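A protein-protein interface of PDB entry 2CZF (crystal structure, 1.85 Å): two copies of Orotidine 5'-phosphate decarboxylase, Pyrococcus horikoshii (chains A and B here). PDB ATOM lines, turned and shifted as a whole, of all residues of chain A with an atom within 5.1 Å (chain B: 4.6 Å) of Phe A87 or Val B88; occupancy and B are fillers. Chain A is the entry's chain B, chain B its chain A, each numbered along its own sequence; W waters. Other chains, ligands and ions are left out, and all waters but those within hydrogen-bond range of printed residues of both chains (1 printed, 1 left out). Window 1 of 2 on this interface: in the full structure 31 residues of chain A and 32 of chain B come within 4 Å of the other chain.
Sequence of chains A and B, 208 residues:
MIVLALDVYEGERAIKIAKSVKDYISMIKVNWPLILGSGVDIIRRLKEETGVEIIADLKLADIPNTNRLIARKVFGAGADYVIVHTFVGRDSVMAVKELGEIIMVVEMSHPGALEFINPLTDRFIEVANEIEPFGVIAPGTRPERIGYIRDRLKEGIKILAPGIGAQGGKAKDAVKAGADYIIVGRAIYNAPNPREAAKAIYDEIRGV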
ATOM      1  N   ALA A  61     -26.646 -23.142  14.544  1.00  0.00           N
ATOM      2  CA  ALA A  61     -25.358 -23.726  14.899  1.00  0.00           C
ATOM      3  C   ALA A  61     -25.508 -25.196  15.254  1.00  0.00           C
ATOM      4  O   ALA A  61     -24.965 -25.655  16.267  1.00  0.00           O
ATOM      5  CB  ALA A  61     -24.773 -22.965  16.095  1.00  0.00           C
ATOM      6  N   HIS A  85     -24.284 -19.302  11.950  1.00  0.00           N
ATOM      7  CA  HIS A  85     -22.934 -19.212  12.495  1.00  0.00           C
ATOM      8  C   HIS A  85     -21.962 -19.930  11.567  1.00  0.00           C
ATOM      9  O   HIS A  85     -22.321 -20.884  10.874  1.00  0.00           O
ATOM     10  CB  HIS A  85     -22.871 -19.862  13.880  1.00  0.00           C
ATOM     11  CG  HIS A  85     -23.098 -18.902  15.003  1.00  0.00           C
ATOM     12  ND1 HIS A  85     -22.244 -17.849  15.263  1.00  0.00           N
ATOM     13  CD2 HIS A  85     -24.072 -18.842  15.943  1.00  0.00           C
ATOM     14  CE1 HIS A  85     -22.684 -17.183  16.319  1.00  0.00           C
ATOM     15  NE2 HIS A  85     -23.790 -17.766  16.750  1.00  0.00           N
ATOM     16  N   THR A  86     -20.723 -19.467  11.565  1.00  0.00           N
ATOM     17  CA  THR A  86     -19.678 -20.058  10.750  1.00  0.00           C
ATOM     18  C   THR A  86     -18.926 -21.082  11.573  1.00  0.00           C
ATOM     19  O   THR A  86     -18.403 -22.048  11.023  1.00  0.00           O
ATOM     20  CB  THR A  86     -18.644 -18.997  10.311  1.00  0.00           C
ATOM     21  OG1 THR A  86     -19.315 -17.929   9.643  1.00  0.00           O
ATOM     22  CG2 THR A  86     -17.619 -19.602   9.374  1.00  0.00           C
ATOM     23  N   PHE A  87     -18.888 -20.893  12.895  1.00  0.00           N
ATOM     24  CA  PHE A  87     -18.105 -21.798  13.732  1.00  0.00           C
ATOM     25  C   PHE A  87     -18.463 -23.263  13.730  1.00  0.00           C
ATOM     26  O   PHE A  87     -17.620 -24.103  14.066  1.00  0.00           O
ATOM     27  CB  PHE A  87     -17.996 -21.288  15.194  1.00  0.00           C
ATOM     28  CG  PHE A  87     -19.248 -21.450  16.039  1.00  0.00           C
ATOM     29  CD1 PHE A  87     -20.088 -20.360  16.296  1.00  0.00           C
ATOM     30  CD2 PHE A  87     -19.511 -22.650  16.708  1.00  0.00           C
ATOM     31  CE1 PHE A  87     -21.164 -20.463  17.221  1.00  0.00           C
ATOM     32  CE2 PHE A  87     -20.585 -22.758  17.635  1.00  0.00           C
ATOM     33  CZ  PHE A  87     -21.400 -21.660  17.886  1.00  0.00           C
ATOM     34  N   VAL A  88     -19.682 -23.600  13.332  1.00  0.00           N
ATOM     35  CA  VAL A  88     -20.071 -25.006  13.345  1.00  0.00           C
ATOM     36  C   VAL A  88     -19.555 -25.759  12.122  1.00  0.00           C
ATOM     37  O   VAL A  88     -19.679 -26.981  12.038  1.00  0.00           O
ATOM     38  CB  VAL A  88     -21.612 -25.157  13.519  1.00  0.00           C
ATOM     39  CG1 VAL A  88     -22.044 -26.616  13.386  1.00  0.00           C
ATOM     40  CG2 VAL A  88     -21.991 -24.679  14.915  1.00  0.00           C
ATOM     41  N   GLY A  89     -18.960 -25.035  11.182  1.00  0.00           N
ATOM     42  CA  GLY A  89     -18.397 -25.701  10.019  1.00  0.00           C
ATOM     43  C   GLY A  89     -19.096 -25.431   8.705  1.00  0.00           C
ATOM     44  O   GLY A  89     -20.258 -25.029   8.679  1.00  0.00           O
ATOM     45  N   MET A 108     -18.622 -11.012  16.608  1.00  0.00           N
ATOM     46  CA  MET A 108     -19.713 -10.538  17.464  1.00  0.00           C
ATOM     47  C   MET A 108     -19.236  -9.400  18.364  1.00  0.00           C
ATOM     48  O   MET A 108     -18.030  -9.168  18.501  1.00  0.00           O
ATOM     49  CB  MET A 108     -20.329 -11.696  18.262  1.00  0.00           C
ATOM     50  CG  MET A 108     -21.104 -12.680  17.360  1.00  0.00           C
ATOM     51  SD  MET A 108     -21.767 -14.138  18.215  1.00  0.00           S
ATOM     52  CE  MET A 108     -23.418 -13.552  18.638  1.00  0.00           C
ATOM     53  N   HIS A 110     -20.536  -8.682  21.795  1.00  0.00           N
ATOM     54  CA  HIS A 110     -20.697  -8.808  23.238  1.00  0.00           C
ATOM     55  C   HIS A 110     -19.334  -9.227  23.801  1.00  0.00           C
ATOM     56  O   HIS A 110     -18.489  -9.755  23.079  1.00  0.00           O
ATOM     57  CB  HIS A 110     -21.771  -9.852  23.558  1.00  0.00           C
ATOM     58  CG  HIS A 110     -21.458 -11.217  23.028  1.00  0.00           C
ATOM     59  ND1 HIS A 110     -21.418 -11.499  21.679  1.00  0.00           N
ATOM     60  CD2 HIS A 110     -21.126 -12.363  23.666  1.00  0.00           C
ATOM     61  CE1 HIS A 110     -21.070 -12.762  21.510  1.00  0.00           C
ATOM     62  NE2 HIS A 110     -20.886 -13.308  22.699  1.00  0.00           N
ATOM     63  N   GLY A 112     -18.328 -11.729  25.606  1.00  0.00           N
ATOM     64  CA  GLY A 112     -18.023 -13.137  25.393  1.00  0.00           C
ATOM     65  C   GLY A 112     -17.433 -13.445  24.027  1.00  0.00           C
ATOM     66  O   GLY A 112     -16.779 -14.471  23.848  1.00  0.00           O
ATOM     67  N   ALA A 113     -17.655 -12.559  23.058  1.00  0.00           N
ATOM     68  CA  ALA A 113     -17.136 -12.757  21.706  1.00  0.00           C
ATOM     69  C   ALA A 113     -15.606 -12.790  21.657  1.00  0.00           C
ATOM     70  O   ALA A 113     -15.020 -13.377  20.746  1.00  0.00           O
ATOM     71  CB  ALA A 113     -17.669 -11.646  20.771  1.00  0.00           C
ATOM     72  N   ILE A 117     -14.900 -16.559  19.345  1.00  0.00           N
ATOM     73  CA  ILE A 117     -15.342 -16.097  18.033  1.00  0.00           C
ATOM     74  C   ILE A 117     -14.438 -15.072  17.354  1.00  0.00           C
ATOM     75  O   ILE A 117     -13.971 -15.309  16.234  1.00  0.00           O
ATOM     76  CB  ILE A 117     -16.775 -15.514  18.083  1.00  0.00           C
ATOM     77  CG1 ILE A 117     -17.766 -16.642  18.377  1.00  0.00           C
ATOM     78  CG2 ILE A 117     -17.145 -14.865  16.732  1.00  0.00           C
ATOM     79  CD1 ILE A 117     -19.181 -16.205  18.416  1.00  0.00           C
ATOM     80  N   PHE A 124     -12.913 -16.887   9.615  1.00  0.00           N
ATOM     81  CA  PHE A 124     -14.322 -16.970   9.261  1.00  0.00           C
ATOM     82  C   PHE A 124     -14.596 -16.189   7.982  1.00  0.00           C
ATOM     83  O   PHE A 124     -15.381 -16.613   7.134  1.00  0.00           O
ATOM     84  CB  PHE A 124     -15.196 -16.455  10.412  1.00  0.00           C
ATOM     85  CG  PHE A 124     -15.223 -17.372  11.604  1.00  0.00           C
ATOM     86  CD1 PHE A 124     -14.944 -18.730  11.458  1.00  0.00           C
ATOM     87  CD2 PHE A 124     -15.548 -16.886  12.864  1.00  0.00           C
ATOM     88  CE1 PHE A 124     -14.987 -19.600  12.562  1.00  0.00           C
ATOM     89  CE2 PHE A 124     -15.595 -17.744  13.972  1.00  0.00           C
ATOM     90  CZ  PHE A 124     -15.313 -19.100  13.819  1.00  0.00           C
ATOM     91  N   ALA B  61     -26.723 -19.722  20.901  1.00  0.00           N
ATOM     92  CA  ALA B  61     -25.467 -19.142  20.479  1.00  0.00           C
ATOM     93  C   ALA B  61     -25.672 -17.686  20.076  1.00  0.00           C
ATOM     94  O   ALA B  61     -25.213 -17.251  19.013  1.00  0.00           O
ATOM     95  CB  ALA B  61     -24.914 -19.928  19.314  1.00  0.00           C
ATOM     96  N   ASP B  62     -26.379 -16.939  20.915  1.00  0.00           N
ATOM     97  CA  ASP B  62     -26.608 -15.534  20.630  1.00  0.00           C
ATOM     98  C   ASP B  62     -26.011 -14.708  21.745  1.00  0.00           C
ATOM     99  O   ASP B  62     -25.360 -15.242  22.643  1.00  0.00           O
ATOM    100  CB  ASP B  62     -28.098 -15.243  20.513  1.00  0.00           C
ATOM    101  CG  ASP B  62     -28.398 -14.135  19.499  1.00  0.00           C
ATOM    102  OD1 ASP B  62     -27.774 -13.050  19.586  1.00  0.00           O
ATOM    103  OD2 ASP B  62     -29.264 -14.355  18.620  1.00  0.00           O
ATOM    104  N   HIS B  85     -24.323 -23.486  23.445  1.00  0.00           N
ATOM    105  CA  HIS B  85     -22.971 -23.630  22.910  1.00  0.00           C
ATOM    106  C   HIS B  85     -22.019 -22.929  23.860  1.00  0.00           C
ATOM    107  O   HIS B  85     -22.420 -22.015  24.570  1.00  0.00           O
ATOM    108  CB  HIS B  85     -22.845 -22.949  21.544  1.00  0.00           C
ATOM    109  CG  HIS B  85     -23.098 -23.861  20.385  1.00  0.00           C
ATOM    110  ND1 HIS B  85     -22.242 -24.889  20.050  1.00  0.00           N
ATOM    111  CD2 HIS B  85     -24.109 -23.903  19.487  1.00  0.00           C
ATOM    112  CE1 HIS B  85     -22.718 -25.529  18.995  1.00  0.00           C
ATOM    113  NE2 HIS B  85     -23.851 -24.951  18.636  1.00  0.00           N
ATOM    114  N   THR B  86     -20.763 -23.351  23.851  1.00  0.00           N
ATOM    115  CA  THR B  86     -19.732 -22.738  24.682  1.00  0.00           C
ATOM    116  C   THR B  86     -19.002 -21.647  23.873  1.00  0.00           C
ATOM    117  O   THR B  86     -18.510 -20.654  24.426  1.00  0.00           O
ATOM    118  CB  THR B  86     -18.666 -23.777  25.099  1.00  0.00           C
ATOM    119  OG1 THR B  86     -19.299 -24.920  25.693  1.00  0.00           O
ATOM    120  CG2 THR B  86     -17.690 -23.167  26.099  1.00  0.00           C
ATOM    121  N   PHE B  87     -18.929 -21.872  22.565  1.00  0.00           N
ATOM    122  CA  PHE B  87     -18.221 -21.009  21.599  1.00  0.00           C
ATOM    123  C   PHE B  87     -18.499 -19.508  21.675  1.00  0.00           C
ATOM    124  O   PHE B  87     -17.592 -18.688  21.504  1.00  0.00           O
ATOM    125  CB  PHE B  87     -18.531 -21.505  20.173  1.00  0.00           C
ATOM    126  CG  PHE B  87     -17.357 -21.455  19.228  1.00  0.00           C
ATOM    127  CD1 PHE B  87     -16.793 -20.238  18.842  1.00  0.00           C
ATOM    128  CD2 PHE B  87     -16.831 -22.638  18.686  1.00  0.00           C
ATOM    129  CE1 PHE B  87     -15.720 -20.197  17.923  1.00  0.00           C
ATOM    130  CE2 PHE B  87     -15.755 -22.605  17.765  1.00  0.00           C
ATOM    131  CZ  PHE B  87     -15.206 -21.383  17.389  1.00  0.00           C
ATOM    132  N   VAL B  88     -19.744 -19.143  21.947  1.00  0.00           N
ATOM    133  CA  VAL B  88     -20.096 -17.737  21.977  1.00  0.00           C
ATOM    134  C   VAL B  88     -19.638 -17.000  23.234  1.00  0.00           C
ATOM    135  O   VAL B  88     -19.761 -15.782  23.315  1.00  0.00           O
ATOM    136  CB  VAL B  88     -21.618 -17.573  21.736  1.00  0.00           C
ATOM    137  CG1 VAL B  88     -22.015 -16.118  21.769  1.00  0.00           C
ATOM    138  CG2 VAL B  88     -21.980 -18.177  20.384  1.00  0.00           C
ATOM    139  N   GLY B  89     -19.099 -17.730  24.212  1.00  0.00           N
ATOM    140  CA  GLY B  89     -18.607 -17.069  25.412  1.00  0.00           C
ATOM    141  C   GLY B  89     -19.318 -17.342  26.723  1.00  0.00           C
ATOM    142  O   GLY B  89     -20.467 -17.787  26.753  1.00  0.00           O
ATOM    143  N   ASP B  91     -20.379 -15.120  29.129  1.00  0.00           N
ATOM    144  CA  ASP B  91     -21.514 -14.282  29.485  1.00  0.00           C
ATOM    145  C   ASP B  91     -22.806 -14.835  28.879  1.00  0.00           C
ATOM    146  O   ASP B  91     -23.855 -14.814  29.518  1.00  0.00           O
ATOM    147  CB  ASP B  91     -21.284 -12.811  29.077  1.00  0.00           C
ATOM    148  CG  ASP B  91     -20.914 -12.636  27.607  1.00  0.00           C
ATOM    149  OD1 ASP B  91     -20.718 -11.464  27.197  1.00  0.00           O
ATOM    150  OD2 ASP B  91     -20.822 -13.639  26.862  1.00  0.00           O
ATOM    151  N   SER B  92     -22.724 -15.372  27.665  1.00  0.00           N
ATOM    152  CA  SER B  92     -23.897 -15.925  27.007  1.00  0.00           C
ATOM    153  C   SER B  92     -24.379 -17.223  27.666  1.00  0.00           C
ATOM    154  O   SER B  92     -25.575 -17.521  27.685  1.00  0.00           O
ATOM    155  CB  SER B  92     -23.597 -16.139  25.522  1.00  0.00           C
ATOM    156  OG  SER B  92     -23.552 -14.876  24.862  1.00  0.00           O
ATOM    157  N   PHE B 116     -13.679 -26.126  13.547  1.00  0.00           N
ATOM    158  CA  PHE B 116     -13.419 -25.139  14.599  1.00  0.00           C
ATOM    159  C   PHE B 116     -13.778 -25.578  16.010  1.00  0.00           C
ATOM    160  O   PHE B 116     -13.074 -25.242  16.958  1.00  0.00           O
ATOM    161  CB  PHE B 116     -14.179 -23.847  14.320  1.00  0.00           C
ATOM    162  CG  PHE B 116     -13.811 -23.196  13.029  1.00  0.00           C
ATOM    163  CD1 PHE B 116     -14.673 -23.249  11.948  1.00  0.00           C
ATOM    164  CD2 PHE B 116     -12.610 -22.512  12.900  1.00  0.00           C
ATOM    165  CE1 PHE B 116     -14.350 -22.621  10.747  1.00  0.00           C
ATOM    166  CE2 PHE B 116     -12.275 -21.880  11.705  1.00  0.00           C
ATOM    167  CZ  PHE B 116     -13.144 -21.934  10.627  1.00  0.00           C
ATOM    168  N   ILE B 117     -14.879 -26.309  16.137  1.00  0.00           N
ATOM    169  CA  ILE B 117     -15.361 -26.762  17.426  1.00  0.00           C
ATOM    170  C   ILE B 117     -14.465 -27.808  18.082  1.00  0.00           C
ATOM    171  O   ILE B 117     -13.912 -27.556  19.152  1.00  0.00           O
ATOM    172  CB  ILE B 117     -16.801 -27.320  17.300  1.00  0.00           C
ATOM    173  CG1 ILE B 117     -17.766 -26.168  16.996  1.00  0.00           C
ATOM    174  CG2 ILE B 117     -17.213 -28.044  18.578  1.00  0.00           C
ATOM    175  CD1 ILE B 117     -19.173 -26.621  16.714  1.00  0.00           C
HETATM  176  O   HOH W   1     -16.594 -26.600  13.524  1.00  0.00           O
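The backbone carbonyl oxygen (O) of Ala A61 sits at hydrogen-bond distance from a ring nitrogen (NE2) of His B85, at 2.7 Å.
The side-chain carboxylate (OD1) of Asp B91 sits at hydrogen-bond distance from the backbone NH (N) of Gly A112 (2.9 Å).
A ring nitrogen (NE2) of His A110 lies within hydrogen-bond range of the backbone carbonyl oxygen (O) of Val B88.
The backbone carbonyl oxygen (O) of Ala B61 sits at hydrogen-bond distance from a ring nitrogen (NE2) of His A85.
O of Gly A112 sits close to O of Val B88, at 3.3 Å.
OG of Ser B92 sits at hydrogen-bond distance from O of Asp B62, at 2.9 Å.
The backbone NH (N) of Ala A113 lies within hydrogen-bond range of a ring nitrogen (NE2) of His A110 (3.3 Å).
His B85 touches Phe A87.
Phe B87 touches Phe A87.
Phe A87 touches Val B88 (CE1 to CG2, 3.99 Å).
Phe A87 touches Phe B116.
CG1 of Ile B117 touches O of Phe A87, at 3.6 Å.
His A110 touches Ser B92.
Val B88 touches Ala A113.
Ile A117 touches Phe B87 (CG1 to O, 3.7 Å).
CD1 of Ile A117 touches CG2 of Val B88 (3.9 Å).
CZ of Phe B116 touches CE1 of Phe A124, at 3.5 Å.
Of the printed residues of chain B, Phe A87 touches His B85 (3.6 Å), Phe B87 (3.3 Å), Val B88 (3.99 Å), Phe B116 (3.5 Å) and Ile B117 (3.6 Å).
Printed residues of chain A within 4 Å of Val B88: Phe A87 (3.99 Å), His A110 (2.8 Å), Gly A112 (3.3 Å), Ala A113 (3.9 Å) and Ile A117 (3.9 Å).
Of the printed residues of chain A, Ser B92 touches His A110.
Of the printed residues of chain B, His A110 touches Val B88 (2.8 Å), Asp B91 (3.5 Å) and Ser B92 (3.7 Å).
Of the printed residues of chain B, Ile A117 touches Phe B87 (3.7 Å) and Val B88 (3.9 Å).
Of the printed residues of chain A, His B85 touches Ala A61 (2.7 Å) and Phe A87 (3.6 Å).
The nearest printed residue of chain A that does not touch Ala B61 is Met A108 (4.1 Å).
Of the 11 printed residues of chain B, 9 touch a printed residue of chain A.
Printed residues of chain B that touch a printed residue of chain A: Ala B61, His B85, Phe B87, Val B88, Gly B89, Asp B91, Ser B92, Phe B116 and Ile B117.
Hydrophobic or aromatic side chains of chain A within 4 Å of the printed part of chain B: Ala A61, His A85, Phe A87, Val A88, His A110, Ile A117 and Phe A124.
Among the printed residues, no Asp or Glu carboxylate lies within 4 Å of a Lys or Arg side-chain nitrogen of the other chain.
Ala A61 touches His B85, and with the chains exchanged His A85 touches Ala B61.
Phe A87 touches His B85, but with the chains exchanged His A85 does not touch Phe B87 (6.9 Å).
Phe A87 touches Val B88, but with the chains exchanged Val A88 does not touch Phe B87 (6.0 Å).
Phe A87 touches Ile B117, and with the chains exchanged Ile A117 touches Phe B87.
7 positions are printed for both chains.
Of the 18 pairs that touch across the chains among the printed residues, 7 have their exchanged pair printed and touching as well.
Water W1 lies within hydrogen-bond range of the backbone carbonyl oxygen (O) of Phe A87 (2.8 Å), the backbone NH (N) of Phe B116 (3.0 Å), the backbone NH (N) of Ile B117 (3.1 Å) and the backbone carbonyl oxygen (O) of Val A88 (3.4 Å).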
